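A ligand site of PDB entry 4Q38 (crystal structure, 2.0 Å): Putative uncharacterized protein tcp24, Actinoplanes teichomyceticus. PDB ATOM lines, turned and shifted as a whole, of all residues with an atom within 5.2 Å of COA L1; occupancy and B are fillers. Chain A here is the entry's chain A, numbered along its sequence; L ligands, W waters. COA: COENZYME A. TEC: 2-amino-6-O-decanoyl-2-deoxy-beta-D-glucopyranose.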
ATOM      1  N   ARG A 193      23.685  11.777 -26.551  1.00  0.00           N
ATOM      2  CA  ARG A 193      23.741  13.236 -26.742  1.00  0.00           C
ATOM      3  C   ARG A 193      25.107  13.703 -27.272  1.00  0.00           C
ATOM      4  O   ARG A 193      25.183  14.676 -28.021  1.00  0.00           O
ATOM      5  CB  ARG A 193      23.400  13.977 -25.428  1.00  0.00           C
ATOM      6  CG  ARG A 193      23.224  15.492 -25.558  1.00  0.00           C
ATOM      7  CD  ARG A 193      22.106  15.809 -26.539  1.00  0.00           C
ATOM      8  NE  ARG A 193      22.032  17.207 -26.974  1.00  0.00           N
ATOM      9  CZ  ARG A 193      22.793  17.779 -27.902  1.00  0.00           C
ATOM     10  NH1 ARG A 193      23.775  17.090 -28.513  1.00  0.00           N
ATOM     11  NH2 ARG A 193      22.600  19.049 -28.227  1.00  0.00           N
ATOM     12  N   VAL A 212      29.838  17.976 -29.231  1.00  0.00           N
ATOM     13  CA  VAL A 212      28.422  18.187 -28.961  1.00  0.00           C
ATOM     14  C   VAL A 212      27.735  18.644 -30.247  1.00  0.00           C
ATOM     15  O   VAL A 212      27.897  19.800 -30.661  1.00  0.00           O
ATOM     16  CB  VAL A 212      28.196  19.228 -27.823  1.00  0.00           C
ATOM     17  CG1 VAL A 212      26.699  19.367 -27.525  1.00  0.00           C
ATOM     18  CG2 VAL A 212      28.947  18.841 -26.550  1.00  0.00           C
ATOM     19  N   PRO A 213      27.008  17.730 -30.901  1.00  0.00           N
ATOM     20  CA  PRO A 213      26.226  18.147 -32.064  1.00  0.00           C
ATOM     21  C   PRO A 213      25.065  19.037 -31.629  1.00  0.00           C
ATOM     22  O   PRO A 213      24.612  18.984 -30.468  1.00  0.00           O
ATOM     23  CB  PRO A 213      25.697  16.822 -32.633  1.00  0.00           C
ATOM     24  CG  PRO A 213      25.781  15.839 -31.515  1.00  0.00           C
ATOM     25  CD  PRO A 213      26.871  16.295 -30.595  1.00  0.00           C
ATOM     26  N   GLU A 214      24.592  19.886 -32.531  1.00  0.00           N
ATOM     27  CA  GLU A 214      23.569  20.848 -32.166  1.00  0.00           C
ATOM     28  C   GLU A 214      22.240  20.137 -31.888  1.00  0.00           C
ATOM     29  O   GLU A 214      21.592  20.390 -30.878  1.00  0.00           O
ATOM     30  CB  GLU A 214      23.390  21.914 -33.251  1.00  0.00           C
ATOM     31  CG  GLU A 214      22.242  22.880 -32.916  1.00  0.00           C
ATOM     32  CD  GLU A 214      22.076  23.967 -33.951  1.00  0.00           C
ATOM     33  OE1 GLU A 214      23.040  24.701 -34.221  1.00  0.00           O
ATOM     34  OE2 GLU A 214      20.960  24.086 -34.496  1.00  0.00           O
ATOM     35  N   GLY A 217      18.465  18.554 -28.552  1.00  0.00           N
ATOM     36  CA  GLY A 217      17.998  19.308 -27.373  1.00  0.00           C
ATOM     37  C   GLY A 217      19.105  19.730 -26.419  1.00  0.00           C
ATOM     38  O   GLY A 217      20.294  19.620 -26.743  1.00  0.00           O
ATOM     39  N   PRO A 218      18.724  20.229 -25.219  1.00  0.00           N
ATOM     40  CA  PRO A 218      19.703  20.732 -24.258  1.00  0.00           C
ATOM     41  C   PRO A 218      20.697  19.679 -23.790  1.00  0.00           C
ATOM     42  O   PRO A 218      20.421  18.477 -23.841  1.00  0.00           O
ATOM     43  CB  PRO A 218      18.840  21.194 -23.073  1.00  0.00           C
ATOM     44  CG  PRO A 218      17.506  21.516 -23.683  1.00  0.00           C
ATOM     45  CD  PRO A 218      17.330  20.495 -24.780  1.00  0.00           C
ATOM     46  N   LEU A 219      21.850  20.141 -23.330  1.00  0.00           N
ATOM     47  CA  LEU A 219      22.884  19.268 -22.799  1.00  0.00           C
ATOM     48  C   LEU A 219      22.540  18.897 -21.349  1.00  0.00           C
ATOM     49  O   LEU A 219      23.246  19.268 -20.412  1.00  0.00           O
ATOM     50  CB  LEU A 219      24.233  19.983 -22.874  1.00  0.00           C
ATOM     51  CG  LEU A 219      25.474  19.281 -23.434  1.00  0.00           C
ATOM     52  CD1 LEU A 219      26.733  19.926 -22.861  1.00  0.00           C
ATOM     53  CD2 LEU A 219      25.480  17.782 -23.165  1.00  0.00           C
ATOM     54  N   LEU A 220      21.436  18.152 -21.179  1.00  0.00           N
ATOM     55  CA  LEU A 220      20.952  17.757 -19.843  1.00  0.00           C
ATOM     56  C   LEU A 220      21.984  16.858 -19.149  1.00  0.00           C
ATOM     57  O   LEU A 220      22.568  15.985 -19.787  1.00  0.00           O
ATOM     58  CB  LEU A 220      19.615  17.021 -19.969  1.00  0.00           C
ATOM     59  CG  LEU A 220      18.369  17.761 -20.524  1.00  0.00           C
ATOM     60  CD1 LEU A 220      17.178  16.810 -20.612  1.00  0.00           C
ATOM     61  CD2 LEU A 220      18.006  18.976 -19.688  1.00  0.00           C
ATOM     62  N   SER A 250      37.796  20.723 -26.632  1.00  0.00           N
ATOM     63  CA  SER A 250      38.179  22.113 -26.843  1.00  0.00           C
ATOM     64  C   SER A 250      36.932  22.851 -27.313  1.00  0.00           C
ATOM     65  O   SER A 250      36.315  22.454 -28.295  1.00  0.00           O
ATOM     66  CB  SER A 250      39.280  22.258 -27.906  1.00  0.00           C
ATOM     67  OG  SER A 250      40.443  21.544 -27.542  1.00  0.00           O
ATOM     68  N   SER A 251      36.540  23.910 -26.605  1.00  0.00           N
ATOM     69  CA  SER A 251      35.268  24.549 -26.911  1.00  0.00           C
ATOM     70  C   SER A 251      35.121  25.931 -26.279  1.00  0.00           C
ATOM     71  O   SER A 251      35.687  26.201 -25.216  1.00  0.00           O
ATOM     72  CB  SER A 251      34.098  23.668 -26.417  1.00  0.00           C
ATOM     73  OG  SER A 251      32.847  24.226 -26.796  1.00  0.00           O
ATOM     74  N   TRP A 252      34.349  26.775 -26.937  1.00  0.00           N
ATOM     75  CA  TRP A 252      33.871  28.013 -26.317  1.00  0.00           C
ATOM     76  C   TRP A 252      33.162  27.733 -25.005  1.00  0.00           C
ATOM     77  O   TRP A 252      33.140  28.594 -24.112  1.00  0.00           O
ATOM     78  CB  TRP A 252      32.958  28.739 -27.290  1.00  0.00           C
ATOM     79  CG  TRP A 252      31.694  27.973 -27.623  1.00  0.00           C
ATOM     80  CD1 TRP A 252      31.480  27.081 -28.677  1.00  0.00           C
ATOM     81  CD2 TRP A 252      30.423  27.999 -26.888  1.00  0.00           C
ATOM     82  NE1 TRP A 252      30.218  26.575 -28.650  1.00  0.00           N
ATOM     83  CE2 TRP A 252      29.518  27.085 -27.609  1.00  0.00           C
ATOM     84  CE3 TRP A 252      29.951  28.656 -25.753  1.00  0.00           C
ATOM     85  CZ2 TRP A 252      28.219  26.862 -27.188  1.00  0.00           C
ATOM     86  CZ3 TRP A 252      28.642  28.418 -25.346  1.00  0.00           C
ATOM     87  CH2 TRP A 252      27.795  27.544 -26.051  1.00  0.00           C
ATOM     88  N   MET A 253      32.602  26.521 -24.879  1.00  0.00           N
ATOM     89  CA  MET A 253      31.790  26.087 -23.723  1.00  0.00           C
ATOM     90  C   MET A 253      32.584  26.002 -22.434  1.00  0.00           C
ATOM     91  O   MET A 253      32.011  26.075 -21.336  1.00  0.00           O
ATOM     92  CB  MET A 253      31.253  24.681 -23.951  1.00  0.00           C
ATOM     93  CG  MET A 253      29.955  24.563 -24.723  1.00  0.00           C
ATOM     94  SD  MET A 253      29.574  22.803 -24.739  1.00  0.00           S
ATOM     95  CE  MET A 253      28.899  22.653 -26.372  1.00  0.00           C
ATOM     96  N   LEU A 262      26.020  33.414 -17.147  1.00  0.00           N
ATOM     97  CA  LEU A 262      25.062  32.316 -17.056  1.00  0.00           C
ATOM     98  C   LEU A 262      24.819  31.954 -15.602  1.00  0.00           C
ATOM     99  O   LEU A 262      25.732  32.028 -14.784  1.00  0.00           O
ATOM    100  CB  LEU A 262      25.553  31.097 -17.833  1.00  0.00           C
ATOM    101  CG  LEU A 262      25.826  31.314 -19.329  1.00  0.00           C
ATOM    102  CD1 LEU A 262      26.366  30.039 -19.970  1.00  0.00           C
ATOM    103  CD2 LEU A 262      24.576  31.803 -20.059  1.00  0.00           C
ATOM    104  N   ASP A 265      21.402  27.410 -13.177  1.00  0.00           N
ATOM    105  CA  ASP A 265      20.549  26.473 -13.904  1.00  0.00           C
ATOM    106  C   ASP A 265      21.139  26.118 -15.287  1.00  0.00           C
ATOM    107  O   ASP A 265      20.657  25.191 -15.930  1.00  0.00           O
ATOM    108  CB  ASP A 265      19.124  27.014 -14.018  1.00  0.00           C
ATOM    109  CG  ASP A 265      19.043  28.308 -14.809  1.00  0.00           C
ATOM    110  OD1 ASP A 265      20.005  29.104 -14.736  1.00  0.00           O
ATOM    111  OD2 ASP A 265      18.024  28.540 -15.490  1.00  0.00           O
ATOM    112  N   SER A 266      22.180  26.836 -15.707  1.00  0.00           N
ATOM    113  CA  SER A 266      22.824  26.555 -16.994  1.00  0.00           C
ATOM    114  C   SER A 266      23.459  25.164 -17.000  1.00  0.00           C
ATOM    115  O   SER A 266      24.192  24.800 -16.080  1.00  0.00           O
ATOM    116  CB  SER A 266      23.871  27.626 -17.322  1.00  0.00           C
ATOM    117  OG  SER A 266      24.791  27.184 -18.321  1.00  0.00           O
ATOM    118  N   ASN A 267      23.136  24.390 -18.027  1.00  0.00           N
ATOM    119  CA  ASN A 267      23.745  23.073 -18.214  1.00  0.00           C
ATOM    120  C   ASN A 267      25.259  23.167 -18.432  1.00  0.00           C
ATOM    121  O   ASN A 267      26.017  22.375 -17.864  1.00  0.00           O
ATOM    122  CB  ASN A 267      23.088  22.350 -19.398  1.00  0.00           C
ATOM    123  CG  ASN A 267      21.637  21.983 -19.114  1.00  0.00           C
ATOM    124  OD1 ASN A 267      21.323  21.574 -18.002  1.00  0.00           O
ATOM    125  ND2 ASN A 267      20.767  22.137 -20.095  1.00  0.00           N
ATOM    126  N   ILE A 268      25.682  24.145 -19.231  1.00  0.00           N
ATOM    127  CA  ILE A 268      27.118  24.396 -19.473  1.00  0.00           C
ATOM    128  C   ILE A 268      27.854  24.639 -18.151  1.00  0.00           C
ATOM    129  O   ILE A 268      28.847  23.954 -17.853  1.00  0.00           O
ATOM    130  CB  ILE A 268      27.322  25.552 -20.481  1.00  0.00           C
ATOM    131  CG1 ILE A 268      26.860  25.095 -21.879  1.00  0.00           C
ATOM    132  CG2 ILE A 268      28.780  26.012 -20.508  1.00  0.00           C
ATOM    133  CD1 ILE A 268      26.713  26.198 -22.916  1.00  0.00           C
ATOM    134  N   ILE A 269      27.345  25.556 -17.334  1.00  0.00           N
ATOM    135  CA  ILE A 269      27.979  25.876 -16.057  1.00  0.00           C
ATOM    136  C   ILE A 269      28.104  24.627 -15.183  1.00  0.00           C
ATOM    137  O   ILE A 269      29.217  24.276 -14.778  1.00  0.00           O
ATOM    138  CB  ILE A 269      27.277  27.041 -15.322  1.00  0.00           C
ATOM    139  CG1 ILE A 269      27.242  28.292 -16.212  1.00  0.00           C
ATOM    140  CG2 ILE A 269      27.967  27.350 -13.994  1.00  0.00           C
ATOM    141  CD1 ILE A 269      28.597  28.880 -16.539  1.00  0.00           C
ATOM    142  N   PHE A 296      28.646  29.166 -33.124  1.00  0.00           N
ATOM    143  CA  PHE A 296      27.776  28.221 -32.421  1.00  0.00           C
ATOM    144  C   PHE A 296      26.562  28.801 -31.702  1.00  0.00           C
ATOM    145  O   PHE A 296      25.573  28.079 -31.472  1.00  0.00           O
ATOM    146  CB  PHE A 296      28.600  27.311 -31.506  1.00  0.00           C
ATOM    147  CG  PHE A 296      29.441  26.352 -32.272  1.00  0.00           C
ATOM    148  CD1 PHE A 296      28.844  25.287 -32.977  1.00  0.00           C
ATOM    149  CD2 PHE A 296      30.824  26.501 -32.332  1.00  0.00           C
ATOM    150  CE1 PHE A 296      29.610  24.398 -33.713  1.00  0.00           C
ATOM    151  CE2 PHE A 296      31.600  25.612 -33.069  1.00  0.00           C
ATOM    152  CZ  PHE A 296      30.993  24.561 -33.759  1.00  0.00           C
ATOM    153  N   VAL A 297      26.606  30.081 -31.376  1.00  0.00           N
ATOM    154  CA  VAL A 297      25.456  30.740 -30.748  1.00  0.00           C
ATOM    155  C   VAL A 297      24.527  31.366 -31.778  1.00  0.00           C
ATOM    156  O   VAL A 297      23.315  31.343 -31.605  1.00  0.00           O
ATOM    157  CB  VAL A 297      25.884  31.756 -29.663  1.00  0.00           C
ATOM    158  CG1 VAL A 297      24.697  32.513 -29.115  1.00  0.00           C
ATOM    159  CG2 VAL A 297      26.591  31.035 -28.527  1.00  0.00           C
ATOM    160  N   ARG A 299      25.332  31.213 -35.554  1.00  0.00           N
ATOM    161  CA  ARG A 299      25.750  30.872 -36.932  1.00  0.00           C
ATOM    162  C   ARG A 299      26.080  32.173 -37.652  1.00  0.00           C
ATOM    163  O   ARG A 299      25.520  32.472 -38.719  1.00  0.00           O
ATOM    164  CB  ARG A 299      24.669  30.077 -37.683  1.00  0.00           C
ATOM    165  CG  ARG A 299      24.293  28.739 -37.052  1.00  0.00           C
ATOM    166  CD  ARG A 299      25.461  27.771 -36.984  1.00  0.00           C
ATOM    167  NE  ARG A 299      25.140  26.645 -36.112  1.00  0.00           N
ATOM    168  CZ  ARG A 299      25.980  25.654 -35.812  1.00  0.00           C
ATOM    169  NH1 ARG A 299      27.202  25.645 -36.314  1.00  0.00           N
ATOM    170  NH2 ARG A 299      25.589  24.679 -34.987  1.00  0.00           N
ATOM    171  N   ARG A 311      17.190  36.637 -27.342  1.00  0.00           N
ATOM    172  CA  ARG A 311      16.149  35.897 -26.638  1.00  0.00           C
ATOM    173  C   ARG A 311      16.649  35.098 -25.425  1.00  0.00           C
ATOM    174  O   ARG A 311      15.961  35.041 -24.395  1.00  0.00           O
ATOM    175  CB  ARG A 311      15.413  34.962 -27.604  1.00  0.00           C
ATOM    176  CG  ARG A 311      14.619  35.681 -28.696  1.00  0.00           C
ATOM    177  CD  ARG A 311      14.259  34.743 -29.843  1.00  0.00           C
ATOM    178  NE  ARG A 311      15.411  34.447 -30.706  1.00  0.00           N
ATOM    179  CZ  ARG A 311      16.169  33.355 -30.613  1.00  0.00           C
ATOM    180  NH1 ARG A 311      15.925  32.426 -29.696  1.00  0.00           N
ATOM    181  NH2 ARG A 311      17.190  33.195 -31.453  1.00  0.00           N
ATOM    182  N   SER A 312      17.826  34.484 -25.543  1.00  0.00           N
ATOM    183  CA  SER A 312      18.357  33.635 -24.462  1.00  0.00           C
ATOM    184  C   SER A 312      19.441  34.357 -23.656  1.00  0.00           C
ATOM    185  O   SER A 312      20.050  35.307 -24.141  1.00  0.00           O
ATOM    186  CB  SER A 312      18.938  32.326 -25.030  1.00  0.00           C
ATOM    187  OG  SER A 312      20.198  32.558 -25.638  1.00  0.00           O
ATOM    188  N   SER A 313      19.701  33.870 -22.434  1.00  0.00           N
ATOM    189  CA  SER A 313      20.739  34.459 -21.598  1.00  0.00           C
ATOM    190  C   SER A 313      22.131  34.413 -22.246  1.00  0.00           C
ATOM    191  O   SER A 313      22.917  35.340 -22.103  1.00  0.00           O
ATOM    192  CB  SER A 313      20.735  33.878 -20.172  1.00  0.00           C
ATOM    193  OG  SER A 313      20.990  32.487 -20.147  1.00  0.00           O
ATOM    194  N   LEU A 314      22.410  33.337 -22.992  1.00  0.00           N
ATOM    195  CA  LEU A 314      23.708  33.205 -23.654  1.00  0.00           C
ATOM    196  C   LEU A 314      23.863  34.155 -24.839  1.00  0.00           C
ATOM    197  O   LEU A 314      24.940  34.727 -25.038  1.00  0.00           O
ATOM    198  CB  LEU A 314      23.943  31.747 -24.090  1.00  0.00           C
ATOM    199  CG  LEU A 314      25.207  31.409 -24.887  1.00  0.00           C
ATOM    200  CD1 LEU A 314      26.458  31.793 -24.133  1.00  0.00           C
ATOM    201  CD2 LEU A 314      25.182  29.924 -25.212  1.00  0.00           C
ATOM    202  N   GLU A 315      22.799  34.315 -25.629  1.00  0.00           N
ATOM    203  CA  GLU A 315      22.789  35.297 -26.719  1.00  0.00           C
ATOM    204  C   GLU A 315      23.094  36.695 -26.190  1.00  0.00           C
ATOM    205  O   GLU A 315      23.906  37.418 -26.778  1.00  0.00           O
ATOM    206  CB  GLU A 315      21.444  35.288 -27.455  1.00  0.00           C
ATOM    207  CG  GLU A 315      21.209  34.062 -28.329  1.00  0.00           C
ATOM    208  CD  GLU A 315      19.775  33.953 -28.831  1.00  0.00           C
ATOM    209  OE1 GLU A 315      18.851  34.496 -28.179  1.00  0.00           O
ATOM    210  OE2 GLU A 315      19.568  33.318 -29.882  1.00  0.00           O
ATOM    211  N   ARG A 316      22.455  37.059 -25.079  1.00  0.00           N
ATOM    212  CA  ARG A 316      22.689  38.369 -24.438  1.00  0.00           C
ATOM    213  C   ARG A 316      24.108  38.455 -23.900  1.00  0.00           C
ATOM    214  O   ARG A 316      24.757  39.490 -24.010  1.00  0.00           O
ATOM    215  CB  ARG A 316      21.655  38.634 -23.339  1.00  0.00           C
ATOM    216  CG  ARG A 316      20.229  38.740 -23.866  1.00  0.00           C
ATOM    217  CD  ARG A 316      19.210  39.200 -22.829  1.00  0.00           C
ATOM    218  NE  ARG A 316      19.027  38.249 -21.726  1.00  0.00           N
ATOM    219  CZ  ARG A 316      18.184  37.214 -21.738  1.00  0.00           C
ATOM    220  NH1 ARG A 316      17.434  36.956 -22.811  1.00  0.00           N
ATOM    221  NH2 ARG A 316      18.093  36.429 -20.670  1.00  0.00           N
HETATM  222  N1A COA L   1      22.360  29.470 -29.005  1.00  0.00           N
HETATM  223  C2A COA L   1      21.502  30.282 -28.347  1.00  0.00           C
HETATM  224  N3A COA L   1      21.163  30.108 -27.057  1.00  0.00           N
HETATM  225  C4A COA L   1      21.686  29.077 -26.341  1.00  0.00           C
HETATM  226  C5A COA L   1      22.616  28.143 -26.995  1.00  0.00           C
HETATM  227  C6A COA L   1      22.944  28.398 -28.417  1.00  0.00           C
HETATM  228  N6A COA L   1      23.806  27.609 -29.111  1.00  0.00           N
HETATM  229  N7A COA L   1      22.958  27.231 -26.059  1.00  0.00           N
HETATM  230  C8A COA L   1      22.315  27.552 -24.921  1.00  0.00           C
HETATM  231  N9A COA L   1      21.539  28.644 -25.097  1.00  0.00           N
HETATM  232  C1B COA L   1      20.693  29.298 -24.067  1.00  0.00           C
HETATM  233  C2B COA L   1      19.718  28.365 -23.387  1.00  0.00           C
HETATM  234  O2B COA L   1      18.491  28.289 -24.116  1.00  0.00           O
HETATM  235  C3B COA L   1      19.574  28.995 -22.024  1.00  0.00           C
HETATM  236  O3B COA L   1      18.736  30.151 -22.151  1.00  0.00           O
HETATM  237  P3B COA L   1      17.930  30.817 -20.910  1.00  0.00           P
HETATM  238  O7A COA L   1      16.815  29.842 -20.673  1.00  0.00           O
HETATM  239  O8A COA L   1      17.556  32.162 -21.472  1.00  0.00           O
HETATM  240  O9A COA L   1      18.915  30.902 -19.773  1.00  0.00           O
HETATM  241  C4B COA L   1      20.991  29.485 -21.733  1.00  0.00           C
HETATM  242  O4B COA L   1      21.551  29.779 -23.015  1.00  0.00           O
HETATM  243  C5B COA L   1      21.867  28.486 -20.982  1.00  0.00           C
HETATM  244  O5B COA L   1      22.033  27.287 -21.761  1.00  0.00           O
HETATM  245  P1A COA L   1      22.682  25.944 -21.178  1.00  0.00           P
HETATM  246  O1A COA L   1      21.708  25.199 -20.318  1.00  0.00           O
HETATM  247  O2A COA L   1      24.026  26.314 -20.619  1.00  0.00           O
HETATM  248  O3A COA L   1      22.939  25.090 -22.536  1.00  0.00           O
HETATM  249  P2A COA L   1      21.877  24.119 -23.257  1.00  0.00           P
HETATM  250  O4A COA L   1      21.987  22.741 -22.647  1.00  0.00           O
HETATM  251  O5A COA L   1      20.517  24.757 -23.340  1.00  0.00           O
HETATM  252  O6A COA L   1      22.486  24.103 -24.741  1.00  0.00           O
HETATM  253  CBP COA L   1      24.003  23.139 -26.422  1.00  0.00           C
HETATM  254  CCP COA L   1      23.803  23.584 -24.979  1.00  0.00           C
HETATM  255  CDP COA L   1      25.452  22.662 -26.509  1.00  0.00           C
HETATM  256  CEP COA L   1      23.051  21.995 -26.717  1.00  0.00           C
HETATM  257  CAP COA L   1      23.754  24.316 -27.391  1.00  0.00           C
HETATM  258  OAP COA L   1      24.554  25.436 -27.018  1.00  0.00           O
HETATM  259  C9P COA L   1      23.993  24.053 -28.871  1.00  0.00           C
HETATM  260  O9P COA L   1      23.181  23.408 -29.518  1.00  0.00           O
HETATM  261  N8P COA L   1      25.090  24.581 -29.414  1.00  0.00           N
HETATM  262  C7P COA L   1      25.528  24.268 -30.766  1.00  0.00           C
HETATM  263  C6P COA L   1      26.507  23.086 -30.768  1.00  0.00           C
HETATM  264  C5P COA L   1      27.796  23.453 -30.054  1.00  0.00           C
HETATM  265  O5P COA L   1      27.990  24.597 -29.668  1.00  0.00           O
HETATM  266  N4P COA L   1      28.657  22.460 -29.849  1.00  0.00           N
HETATM  267  C3P COA L   1      30.025  22.679 -29.395  1.00  0.00           C
HETATM  268  C2P COA L   1      30.947  23.185 -30.496  1.00  0.00           C
HETATM  269  S1P COA L   1      32.634  23.448 -29.840  1.00  0.00           S
HETATM  270  CAV TEC L   2      30.486  21.703 -20.617  1.00  0.00           C
HETATM  271  CAU TEC L   2      30.123  20.493 -21.449  1.00  0.00           C
HETATM  272  CAT TEC L   2      31.337  19.781 -21.985  1.00  0.00           C
HETATM  273  CAS TEC L   2      32.353  20.728 -22.540  1.00  0.00           C
HETATM  274  CAR TEC L   2      33.205  20.018 -23.558  1.00  0.00           C
HETATM  275  CAQ TEC L   2      32.821  20.525 -24.896  1.00  0.00           C
HETATM  276  CAP TEC L   2      33.604  19.925 -26.004  1.00  0.00           C
HETATM  277  CAO TEC L   2      32.826  20.209 -27.248  1.00  0.00           C
HETATM  278  CAN TEC L   2      33.709  20.274 -28.440  1.00  0.00           C
HETATM  279  CAM TEC L   2      32.923  20.288 -29.717  1.00  0.00           C
HETATM  280  OAW TEC L   2      31.725  20.144 -29.717  1.00  0.00           O
HETATM  281  O6  TEC L   2      33.652  20.613 -30.795  1.00  0.00           O
HETATM  282  C6  TEC L   2      33.621  19.805 -31.959  1.00  0.00           C
HETATM  283  C5  TEC L   2      33.023  20.574 -33.169  1.00  0.00           C
HETATM  284  O5  TEC L   2      33.817  20.458 -34.312  1.00  0.00           O
HETATM  285  C1  TEC L   2      33.291  21.576 -35.083  1.00  0.00           C
HETATM  286  O1  TEC L   2      34.089  22.219 -35.885  1.00  0.00           O
HETATM  287  C2  TEC L   2      32.083  21.075 -35.822  1.00  0.00           C
HETATM  288  N2  TEC L   2      31.548  22.178 -36.592  1.00  0.00           N
HETATM  289  C3  TEC L   2      31.169  20.811 -34.717  1.00  0.00           C
HETATM  290  O3  TEC L   2      30.284  20.081 -35.365  1.00  0.00           O
HETATM  291  C4  TEC L   2      31.724  19.991 -33.581  1.00  0.00           C
HETATM  292  O4  TEC L   2      30.947  20.125 -32.553  1.00  0.00           O
HETATM  293  O   HOH W   1      19.431  26.138 -19.199  1.00  0.00           O
HETATM  294  O   HOH W   2      21.678  28.833 -31.762  1.00  0.00           O
HETATM  295  O   HOH W   3      34.550  26.240 -29.954  1.00  0.00           O
HETATM  296  O   HOH W   4      18.451  24.903 -21.867  1.00  0.00           O
HETATM  297  O   HOH W   5      19.795  28.811 -18.104  1.00  0.00           O
HETATM  298  O   HOH W   6      19.304  24.786 -25.731  1.00  0.00           O
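OG of Ser 266 lies within hydrogen-bond range of O2A of COA L1. An oxygen (O8A) of COA L1 is in hydrogen-bond range of the backbone NH (N) of Ser 313 (2.9 Å). OG of Ser 313 lies within hydrogen-bond range of O9A of COA L1, at 2.6 Å. N of Leu 219 sits at hydrogen-bond distance from O4A of COA L1 (2.7 Å). An oxygen (O1A) of COA L1 is in hydrogen-bond range of the backbone NH (N) of Asn 267, 2.8 Å away. O4A of COA L1 sits at hydrogen-bond distance from ND2 of Asn 267. A nitrogen (N4P) of COA L1 is in hydrogen-bond range of the backbone carbonyl oxygen (O) of Val 212 (2.9 Å). O of Phe 296 is in hydrogen-bond range of N6A of COA L1, 3.0 Å away. A nitrogen (N3A) of COA L1 is in hydrogen-bond range of the side-chain hydroxyl (OG) of Ser 312 (3.0 Å). The backbone NH of Ile 268 lies within hydrogen-bond range of an oxygen (O2A) of COA L1, at 3.1 Å. OG of Ser 251 lies close to S1P of COA L1 (3.1 Å). The indole nitrogen (NE1) of Trp 252 sits at hydrogen-bond distance from an oxygen (O5P) of COA L1, 3.1 Å away. The backbone NH of Val 212 lies within hydrogen-bond range of an oxygen (OAW) of TEC L2.
Water W5 bridges an oxygen (O9A) of COA L1 and the side-chain carboxylate of Asp 265. Water W2 lies within hydrogen-bond range of N1A of COA L1 (2.9 Å) and O of Val 297 (3.0 Å). Water W3 bridges N of Trp 252 and S1P of COA L1.
O of Val 297 sits close to N1A of COA L1 (3.3 Å). Merely in contact with COA L1: Met 253 (3.2 Å), Leu 314 (3.3 Å), Arg 193 (3.3 Å), Pro 218 (3.4 Å), Glu 214 (3.6 Å), Gly 217 (3.6 Å) and Glu 315 (3.8 Å). Hydrophobic or aromatic side chains within 4 Å of COA L1: Val 212, Pro 218, Leu 219, Trp 252, Met 253, Ile 268, Phe 296, Val 297 and Leu 314. Of the 27 residues printed, 18 come within 4 Å of COA L1.
OG of Ser 266 sits at hydrogen-bond distance from N of Ile 268 (3.3 Å). The side-chain hydroxyl (OG) of Ser 266 lies within hydrogen-bond range of the backbone NH (N) of Ile 269, at 3.2 Å. OE1 of Glu 315 lies within hydrogen-bond range of N of Ser 312 (2.8 Å). The backbone carbonyl oxygen of Ser 312 lies within hydrogen-bond range of the guanidinium group of Arg 316, 3.4 Å away. The backbone NH (N) of Met 253 lies close to the side-chain hydroxyl (OG) of Ser 251. The guanidinium group of Arg 193 sits at hydrogen-bond distance from the backbone carbonyl oxygen of Glu 214, at 3.1 Å. NH2 of Arg 193 is in hydrogen-bond range of O of Gly 217. NH2 of Arg 299 lies within salt-bridge range of OE1 of Glu 214.
An oxygen (O6) of TEC L2 sits close to a sulfur (S1P) of COA L1.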
